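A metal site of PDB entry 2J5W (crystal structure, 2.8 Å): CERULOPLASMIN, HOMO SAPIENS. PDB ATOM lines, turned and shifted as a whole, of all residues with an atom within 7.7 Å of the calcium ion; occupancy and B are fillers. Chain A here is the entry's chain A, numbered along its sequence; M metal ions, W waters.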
ATOM      1  N   TYR A 127      -2.743  16.183  -1.712  1.00  0.00           N
ATOM      2  CA  TYR A 127      -1.773  16.736  -2.638  1.00  0.00           C
ATOM      3  C   TYR A 127      -0.798  15.615  -2.996  1.00  0.00           C
ATOM      4  O   TYR A 127      -0.836  14.542  -2.382  1.00  0.00           O
ATOM      5  CB  TYR A 127      -1.013  17.877  -1.987  1.00  0.00           C
ATOM      6  CG  TYR A 127      -1.849  19.075  -1.601  1.00  0.00           C
ATOM      7  CD1 TYR A 127      -2.414  19.910  -2.580  1.00  0.00           C
ATOM      8  CD2 TYR A 127      -2.031  19.426  -0.261  1.00  0.00           C
ATOM      9  CE1 TYR A 127      -3.158  21.054  -2.220  1.00  0.00           C
ATOM     10  CE2 TYR A 127      -2.784  20.561   0.108  1.00  0.00           C
ATOM     11  CZ  TYR A 127      -3.331  21.363  -0.875  1.00  0.00           C
ATOM     12  OH  TYR A 127      -4.067  22.463  -0.524  1.00  0.00           O
ATOM     13  N   LYS A 128       0.090  15.859  -3.951  1.00  0.00           N
ATOM     14  CA  LYS A 128       1.078  14.852  -4.367  1.00  0.00           C
ATOM     15  C   LYS A 128       1.956  14.370  -3.197  1.00  0.00           C
ATOM     16  O   LYS A 128       2.403  13.217  -3.207  1.00  0.00           O
ATOM     17  CB  LYS A 128       1.945  15.367  -5.519  1.00  0.00           C
ATOM     18  CG  LYS A 128       1.226  15.572  -6.875  1.00  0.00           C
ATOM     19  CD  LYS A 128       0.632  14.272  -7.499  1.00  0.00           C
ATOM     20  CE  LYS A 128       1.689  13.246  -7.916  1.00  0.00           C
ATOM     21  NZ  LYS A 128       1.100  11.949  -8.355  1.00  0.00           N
ATOM     22  N   GLU A 129       2.180  15.245  -2.204  1.00  0.00           N
ATOM     23  CA  GLU A 129       2.919  14.889  -0.972  1.00  0.00           C
ATOM     24  C   GLU A 129       2.214  13.849  -0.111  1.00  0.00           C
ATOM     25  O   GLU A 129       2.796  13.341   0.819  1.00  0.00           O
ATOM     26  CB  GLU A 129       3.082  16.098  -0.046  1.00  0.00           C
ATOM     27  CG  GLU A 129       3.613  17.342  -0.676  1.00  0.00           C
ATOM     28  CD  GLU A 129       2.532  18.313  -1.099  1.00  0.00           C
ATOM     29  OE1 GLU A 129       1.858  18.877  -0.213  1.00  0.00           O
ATOM     30  OE2 GLU A 129       2.353  18.520  -2.316  1.00  0.00           O
ATOM     31  N   HIS A 130       0.922  13.617  -0.367  1.00  0.00           N
ATOM     32  CA  HIS A 130       0.100  12.821   0.547  1.00  0.00           C
ATOM     33  C   HIS A 130      -0.720  11.738  -0.187  1.00  0.00           C
ATOM     34  O   HIS A 130      -1.744  11.300   0.327  1.00  0.00           O
ATOM     35  CB  HIS A 130      -0.838  13.749   1.334  1.00  0.00           C
ATOM     36  CG  HIS A 130      -0.123  14.767   2.167  1.00  0.00           C
ATOM     37  ND1 HIS A 130      -0.349  16.119   2.042  1.00  0.00           N
ATOM     38  CD2 HIS A 130       0.793  14.632   3.149  1.00  0.00           C
ATOM     39  CE1 HIS A 130       0.399  16.772   2.912  1.00  0.00           C
ATOM     40  NE2 HIS A 130       1.099  15.892   3.598  1.00  0.00           N
ATOM     41  N   GLU A 131      -0.250  11.322  -1.368  1.00  0.00           N
ATOM     42  CA  GLU A 131      -0.900  10.300  -2.181  1.00  0.00           C
ATOM     43  C   GLU A 131      -0.423   8.906  -1.828  1.00  0.00           C
ATOM     44  O   GLU A 131      -1.135   7.940  -2.031  1.00  0.00           O
ATOM     45  CB  GLU A 131      -0.661  10.553  -3.672  1.00  0.00           C
ATOM     46  CG  GLU A 131      -1.072   9.430  -4.640  1.00  0.00           C
ATOM     47  CD  GLU A 131      -0.930   9.810  -6.099  1.00  0.00           C
ATOM     48  OE1 GLU A 131      -0.261  10.830  -6.378  1.00  0.00           O
ATOM     49  OE2 GLU A 131      -1.479   9.102  -6.977  1.00  0.00           O
ATOM     50  N   GLY A 132       0.791   8.806  -1.312  1.00  0.00           N
ATOM     51  CA  GLY A 132       1.372   7.504  -0.939  1.00  0.00           C
ATOM     52  C   GLY A 132       1.410   6.469  -2.052  1.00  0.00           C
ATOM     53  O   GLY A 132       1.219   5.286  -1.802  1.00  0.00           O
ATOM     54  N   ALA A 133       1.666   6.907  -3.281  1.00  0.00           N
ATOM     55  CA  ALA A 133       1.742   6.015  -4.435  1.00  0.00           C
ATOM     56  C   ALA A 133       2.926   6.447  -5.311  1.00  0.00           C
ATOM     57  O   ALA A 133       3.080   7.626  -5.623  1.00  0.00           O
ATOM     58  CB  ALA A 133       0.446   6.030  -5.214  1.00  0.00           C
ATOM     59  N   ILE A 134       3.772   5.485  -5.663  1.00  0.00           N
ATOM     60  CA  ILE A 134       4.970   5.776  -6.437  1.00  0.00           C
ATOM     61  C   ILE A 134       4.741   5.418  -7.909  1.00  0.00           C
ATOM     62  O   ILE A 134       4.355   4.294  -8.243  1.00  0.00           O
ATOM     63  CB  ILE A 134       6.211   5.027  -5.877  1.00  0.00           C
ATOM     64  CG1 ILE A 134       7.491   5.773  -6.284  1.00  0.00           C
ATOM     65  CG2 ILE A 134       6.264   3.562  -6.316  1.00  0.00           C
ATOM     66  CD1 ILE A 134       8.695   5.449  -5.390  1.00  0.00           C
ATOM     67  N   TYR A 135       4.942   6.418  -8.771  1.00  0.00           N
ATOM     68  CA  TYR A 135       4.887   6.247 -10.209  1.00  0.00           C
ATOM     69  C   TYR A 135       5.456   7.516 -10.850  1.00  0.00           C
ATOM     70  O   TYR A 135       5.568   8.535 -10.177  1.00  0.00           O
ATOM     71  CB  TYR A 135       3.464   5.981 -10.691  1.00  0.00           C
ATOM     72  CG  TYR A 135       2.412   6.988 -10.265  1.00  0.00           C
ATOM     73  CD1 TYR A 135       1.786   6.890  -9.033  1.00  0.00           C
ATOM     74  CD2 TYR A 135       2.034   8.031 -11.107  1.00  0.00           C
ATOM     75  CE1 TYR A 135       0.802   7.824  -8.637  1.00  0.00           C
ATOM     76  CE2 TYR A 135       1.064   8.960 -10.738  1.00  0.00           C
ATOM     77  CZ  TYR A 135       0.450   8.850  -9.506  1.00  0.00           C
ATOM     78  OH  TYR A 135      -0.523   9.765  -9.164  1.00  0.00           O
ATOM     79  N   ASP A 137       5.430  10.756 -12.041  1.00  0.00           N
ATOM     80  CA  ASP A 137       4.541  11.911 -12.040  1.00  0.00           C
ATOM     81  C   ASP A 137       5.312  13.245 -12.149  1.00  0.00           C
ATOM     82  O   ASP A 137       4.746  14.309 -11.922  1.00  0.00           O
ATOM     83  CB  ASP A 137       3.684  11.897 -10.766  1.00  0.00           C
ATOM     84  CG  ASP A 137       4.496  11.667  -9.525  1.00  0.00           C
ATOM     85  OD1 ASP A 137       5.705  11.984  -9.546  1.00  0.00           O
ATOM     86  OD2 ASP A 137       3.954  11.152  -8.530  1.00  0.00           O
ATOM     87  N   THR A 139       7.317  14.394 -10.120  1.00  0.00           N
ATOM     88  CA  THR A 139       7.431  15.067  -8.833  1.00  0.00           C
ATOM     89  C   THR A 139       8.883  15.046  -8.338  1.00  0.00           C
ATOM     90  O   THR A 139       9.708  14.221  -8.756  1.00  0.00           O
ATOM     91  CB  THR A 139       6.467  14.473  -7.753  1.00  0.00           C
ATOM     92  OG1 THR A 139       6.733  13.085  -7.554  1.00  0.00           O
ATOM     93  CG2 THR A 139       5.034  14.676  -8.150  1.00  0.00           C
ATOM     94  N   THR A 140       9.211  15.985  -7.457  1.00  0.00           N
ATOM     95  CA  THR A 140      10.521  16.065  -6.869  1.00  0.00           C
ATOM     96  C   THR A 140      10.429  15.575  -5.419  1.00  0.00           C
ATOM     97  O   THR A 140       9.348  15.210  -4.948  1.00  0.00           O
ATOM     98  CB  THR A 140      11.045  17.482  -6.963  1.00  0.00           C
ATOM     99  OG1 THR A 140      10.119  18.368  -6.334  1.00  0.00           O
ATOM    100  CG2 THR A 140      11.208  17.912  -8.415  1.00  0.00           C
ATOM    101  N   ASP A 141      11.560  15.569  -4.727  1.00  0.00           N
ATOM    102  CA  ASP A 141      11.709  14.930  -3.419  1.00  0.00           C
ATOM    103  C   ASP A 141      10.695  15.302  -2.372  1.00  0.00           C
ATOM    104  O   ASP A 141      10.303  14.448  -1.584  1.00  0.00           O
ATOM    105  CB  ASP A 141      13.079  15.256  -2.835  1.00  0.00           C
ATOM    106  CG  ASP A 141      14.187  14.604  -3.601  1.00  0.00           C
ATOM    107  OD1 ASP A 141      14.178  13.362  -3.709  1.00  0.00           O
ATOM    108  OD2 ASP A 141      15.051  15.349  -4.090  1.00  0.00           O
ATOM    109  N   PHE A 142      10.299  16.565  -2.328  1.00  0.00           N
ATOM    110  CA  PHE A 142       9.333  16.996  -1.334  1.00  0.00           C
ATOM    111  C   PHE A 142       8.034  16.221  -1.479  1.00  0.00           C
ATOM    112  O   PHE A 142       7.403  15.858  -0.492  1.00  0.00           O
ATOM    113  CB  PHE A 142       8.997  18.488  -1.428  1.00  0.00           C
ATOM    114  CG  PHE A 142       7.892  18.899  -0.475  1.00  0.00           C
ATOM    115  CD1 PHE A 142       7.964  18.533   0.902  1.00  0.00           C
ATOM    116  CD2 PHE A 142       6.778  19.607  -0.921  1.00  0.00           C
ATOM    117  CE1 PHE A 142       6.927  18.871   1.825  1.00  0.00           C
ATOM    118  CE2 PHE A 142       5.730  19.967   0.000  1.00  0.00           C
ATOM    119  CZ  PHE A 142       5.808  19.600   1.384  1.00  0.00           C
ATOM    120  N   GLN A 143       7.637  15.954  -2.726  1.00  0.00           N
ATOM    121  CA  GLN A 143       6.376  15.289  -3.001  1.00  0.00           C
ATOM    122  C   GLN A 143       6.516  13.782  -3.210  1.00  0.00           C
ATOM    123  O   GLN A 143       5.581  13.134  -3.672  1.00  0.00           O
ATOM    124  CB  GLN A 143       5.741  15.950  -4.211  1.00  0.00           C
ATOM    125  CG  GLN A 143       5.488  17.410  -3.998  1.00  0.00           C
ATOM    126  CD  GLN A 143       4.850  18.053  -5.192  1.00  0.00           C
ATOM    127  OE1 GLN A 143       5.398  18.012  -6.310  1.00  0.00           O
ATOM    128  NE2 GLN A 143       3.678  18.661  -4.974  1.00  0.00           N
ATOM    129  N   ARG A 144       7.664  13.237  -2.814  1.00  0.00           N
ATOM    130  CA  ARG A 144       8.015  11.818  -3.001  1.00  0.00           C
ATOM    131  C   ARG A 144       8.287  11.081  -1.707  1.00  0.00           C
ATOM    132  O   ARG A 144       8.455   9.868  -1.740  1.00  0.00           O
ATOM    133  CB  ARG A 144       9.245  11.705  -3.882  1.00  0.00           C
ATOM    134  CG  ARG A 144       8.935  11.552  -5.340  1.00  0.00           C
ATOM    135  CD  ARG A 144       8.666  10.116  -5.697  1.00  0.00           C
ATOM    136  NE  ARG A 144       8.098   9.981  -7.025  1.00  0.00           N
ATOM    137  CZ  ARG A 144       8.785   9.911  -8.159  1.00  0.00           C
ATOM    138  NH1 ARG A 144      10.103   9.963  -8.167  1.00  0.00           N
ATOM    139  NH2 ARG A 144       8.138   9.788  -9.314  1.00  0.00           N
ATOM    140  N   ALA A 145       8.344  11.791  -0.579  1.00  0.00           N
ATOM    141  CA  ALA A 145       8.544  11.156   0.733  1.00  0.00           C
ATOM    142  C   ALA A 145       7.388  10.223   1.065  1.00  0.00           C
ATOM    143  O   ALA A 145       7.582   9.143   1.606  1.00  0.00           O
ATOM    144  CB  ALA A 145       8.698  12.195   1.830  1.00  0.00           C
ATOM    145  N   ASP A 146       6.177  10.651   0.723  1.00  0.00           N
ATOM    146  CA  ASP A 146       4.982   9.829   0.936  1.00  0.00           C
ATOM    147  C   ASP A 146       5.026   8.462   0.242  1.00  0.00           C
ATOM    148  O   ASP A 146       4.421   7.511   0.716  1.00  0.00           O
ATOM    149  CB  ASP A 146       3.709  10.568   0.514  1.00  0.00           C
ATOM    150  CG  ASP A 146       3.750  11.054  -0.940  1.00  0.00           C
ATOM    151  OD1 ASP A 146       4.842  11.298  -1.469  1.00  0.00           O
ATOM    152  OD2 ASP A 146       2.667  11.197  -1.552  1.00  0.00           O
ATOM    153  N   ASP A 147       5.790   8.370  -0.843  1.00  0.00           N
ATOM    154  CA  ASP A 147       5.702   7.260  -1.791  1.00  0.00           C
ATOM    155  C   ASP A 147       6.593   6.060  -1.515  1.00  0.00           C
ATOM    156  O   ASP A 147       6.436   5.012  -2.140  1.00  0.00           O
ATOM    157  CB  ASP A 147       5.947   7.820  -3.185  1.00  0.00           C
ATOM    158  CG  ASP A 147       5.038   8.999  -3.485  1.00  0.00           C
ATOM    159  OD1 ASP A 147       3.911   9.036  -2.934  1.00  0.00           O
ATOM    160  OD2 ASP A 147       5.431   9.910  -4.230  1.00  0.00           O
ATOM    161  N   LYS A 148       7.521   6.194  -0.560  1.00  0.00           N
ATOM    162  CA  LYS A 148       8.362   5.080  -0.143  1.00  0.00           C
ATOM    163  C   LYS A 148       8.795   5.299   1.315  1.00  0.00           C
ATOM    164  O   LYS A 148       9.814   5.922   1.584  1.00  0.00           O
ATOM    165  CB  LYS A 148       9.578   4.928  -1.098  1.00  0.00           C
ATOM    166  CG  LYS A 148      10.390   3.633  -0.928  1.00  0.00           C
ATOM    167  CD  LYS A 148      11.637   3.552  -1.858  1.00  0.00           C
ATOM    168  CE  LYS A 148      11.281   3.151  -3.311  1.00  0.00           C
ATOM    169  NZ  LYS A 148      12.413   3.248  -4.308  1.00  0.00           N
ATOM    170  N   TYR A 155       5.610   8.890   8.395  1.00  0.00           N
ATOM    171  CA  TYR A 155       5.088   9.971   7.547  1.00  0.00           C
ATOM    172  C   TYR A 155       3.644  10.249   7.940  1.00  0.00           C
ATOM    173  O   TYR A 155       2.861   9.341   8.267  1.00  0.00           O
ATOM    174  CB  TYR A 155       5.185   9.602   6.063  1.00  0.00           C
ATOM    175  CG  TYR A 155       5.007  10.781   5.124  1.00  0.00           C
ATOM    176  CD1 TYR A 155       6.088  11.578   4.769  1.00  0.00           C
ATOM    177  CD2 TYR A 155       3.762  11.095   4.583  1.00  0.00           C
ATOM    178  CE1 TYR A 155       5.934  12.652   3.906  1.00  0.00           C
ATOM    179  CE2 TYR A 155       3.602  12.171   3.727  1.00  0.00           C
ATOM    180  CZ  TYR A 155       4.694  12.938   3.390  1.00  0.00           C
ATOM    181  OH  TYR A 155       4.554  14.002   2.542  1.00  0.00           O
ATOM    182  N   TYR A 157       0.206  11.721   6.672  1.00  0.00           N
ATOM    183  CA  TYR A 157      -0.588  12.072   5.515  1.00  0.00           C
ATOM    184  C   TYR A 157      -1.728  13.006   5.918  1.00  0.00           C
ATOM    185  O   TYR A 157      -2.491  12.689   6.826  1.00  0.00           O
ATOM    186  CB  TYR A 157      -1.177  10.812   4.886  1.00  0.00           C
ATOM    187  CG  TYR A 157      -0.166   9.846   4.342  1.00  0.00           C
ATOM    188  CD1 TYR A 157       0.495   8.962   5.187  1.00  0.00           C
ATOM    189  CD2 TYR A 157       0.116   9.786   2.982  1.00  0.00           C
ATOM    190  CE1 TYR A 157       1.413   8.042   4.684  1.00  0.00           C
ATOM    191  CE2 TYR A 157       1.027   8.866   2.472  1.00  0.00           C
ATOM    192  CZ  TYR A 157       1.677   8.005   3.329  1.00  0.00           C
ATOM    193  OH  TYR A 157       2.605   7.097   2.846  1.00  0.00           O
ATOM    194  N   TRP A1036      -1.600  12.421 -12.382  1.00  0.00           N
ATOM    195  CA  TRP A1036      -2.286  11.424 -11.556  1.00  0.00           C
ATOM    196  C   TRP A1036      -2.456  10.121 -12.284  1.00  0.00           C
ATOM    197  O   TRP A1036      -2.806  10.094 -13.435  1.00  0.00           O
ATOM    198  CB  TRP A1036      -3.657  11.947 -11.169  1.00  0.00           C
ATOM    199  CG  TRP A1036      -3.597  13.217 -10.411  1.00  0.00           C
ATOM    200  CD1 TRP A1036      -3.910  14.465 -10.868  1.00  0.00           C
ATOM    201  CD2 TRP A1036      -3.219  13.369  -9.056  1.00  0.00           C
ATOM    202  NE1 TRP A1036      -3.758  15.390  -9.871  1.00  0.00           N
ATOM    203  CE2 TRP A1036      -3.330  14.744  -8.746  1.00  0.00           C
ATOM    204  CE3 TRP A1036      -2.816  12.487  -8.050  1.00  0.00           C
ATOM    205  CZ2 TRP A1036      -3.038  15.251  -7.474  1.00  0.00           C
ATOM    206  CZ3 TRP A1036      -2.526  12.982  -6.791  1.00  0.00           C
ATOM    207  CH2 TRP A1036      -2.631  14.352  -6.516  1.00  0.00           C
HETATM  208 CA    CA M   1       3.838  11.418  -3.736  1.00  0.00          CA
HETATM  209  O   HOH W   1       2.463  10.218  -5.180  1.00  0.00           O
HETATM  210  O   HOH W   2       4.457  12.269  -6.046  1.00  0.00           O
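NE2 of Gln 143 lies within hydrogen-bond range of OE2 of Glu 129, at 3.0 Å. The side-chain carboxylate (OD1) of Asp 147 sits close to the backbone NH (N) of Ala 133. OD2 of Asp 146 lies close to N of Gly 132 (3.0 Å). N of Glu 131 sits close to OD2 of Asp 146 (2.9 Å). The guanidinium group of Arg 144 sits close to the side-chain carboxylate of Asp 147, at 3.9 Å. NZ of Lys 128 lies within salt-bridge range of OE1 of Glu 131 (2.6 Å). The side-chain carboxylate (OD2) of Asp 137 is in salt-bridge range of the side-chain amino group (NZ) of Lys 128, 3.0 Å away. OH of Tyr 157 lies within hydrogen-bond range of O of Asp 146 (2.8 Å).
Of the 23 residues printed, 4 come within 4 Å of the calcium ion. The nearest printed residue that does not touch the calcium ion is Arg 144 (4.3 Å).
The calcium ion is bound by OD2 of Asp 147 (2.2 Å), water W1 (2.3 Å), O of Lys 128 (2.4 Å), O of Gln 143 (2.4 Å), OD1 of Asp 146 (2.5 Å), OD2 of Asp 146 (2.5 Å), OD1 of Asp 147 (2.5 Å) and water W2 (2.5 Å). The calcium ion has eight donor atoms within binding distance.
Water W1 lies within hydrogen-bond range of the backbone carbonyl oxygen (O) of Ala 133 and the side-chain carboxylate (OE1) of Glu 131. Water W2 lies within hydrogen-bond range of the side-chain carboxylate (OD2) of Asp 137 (2.8 Å) and the side-chain hydroxyl (OG1) of Thr 139 (2.8 Å).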
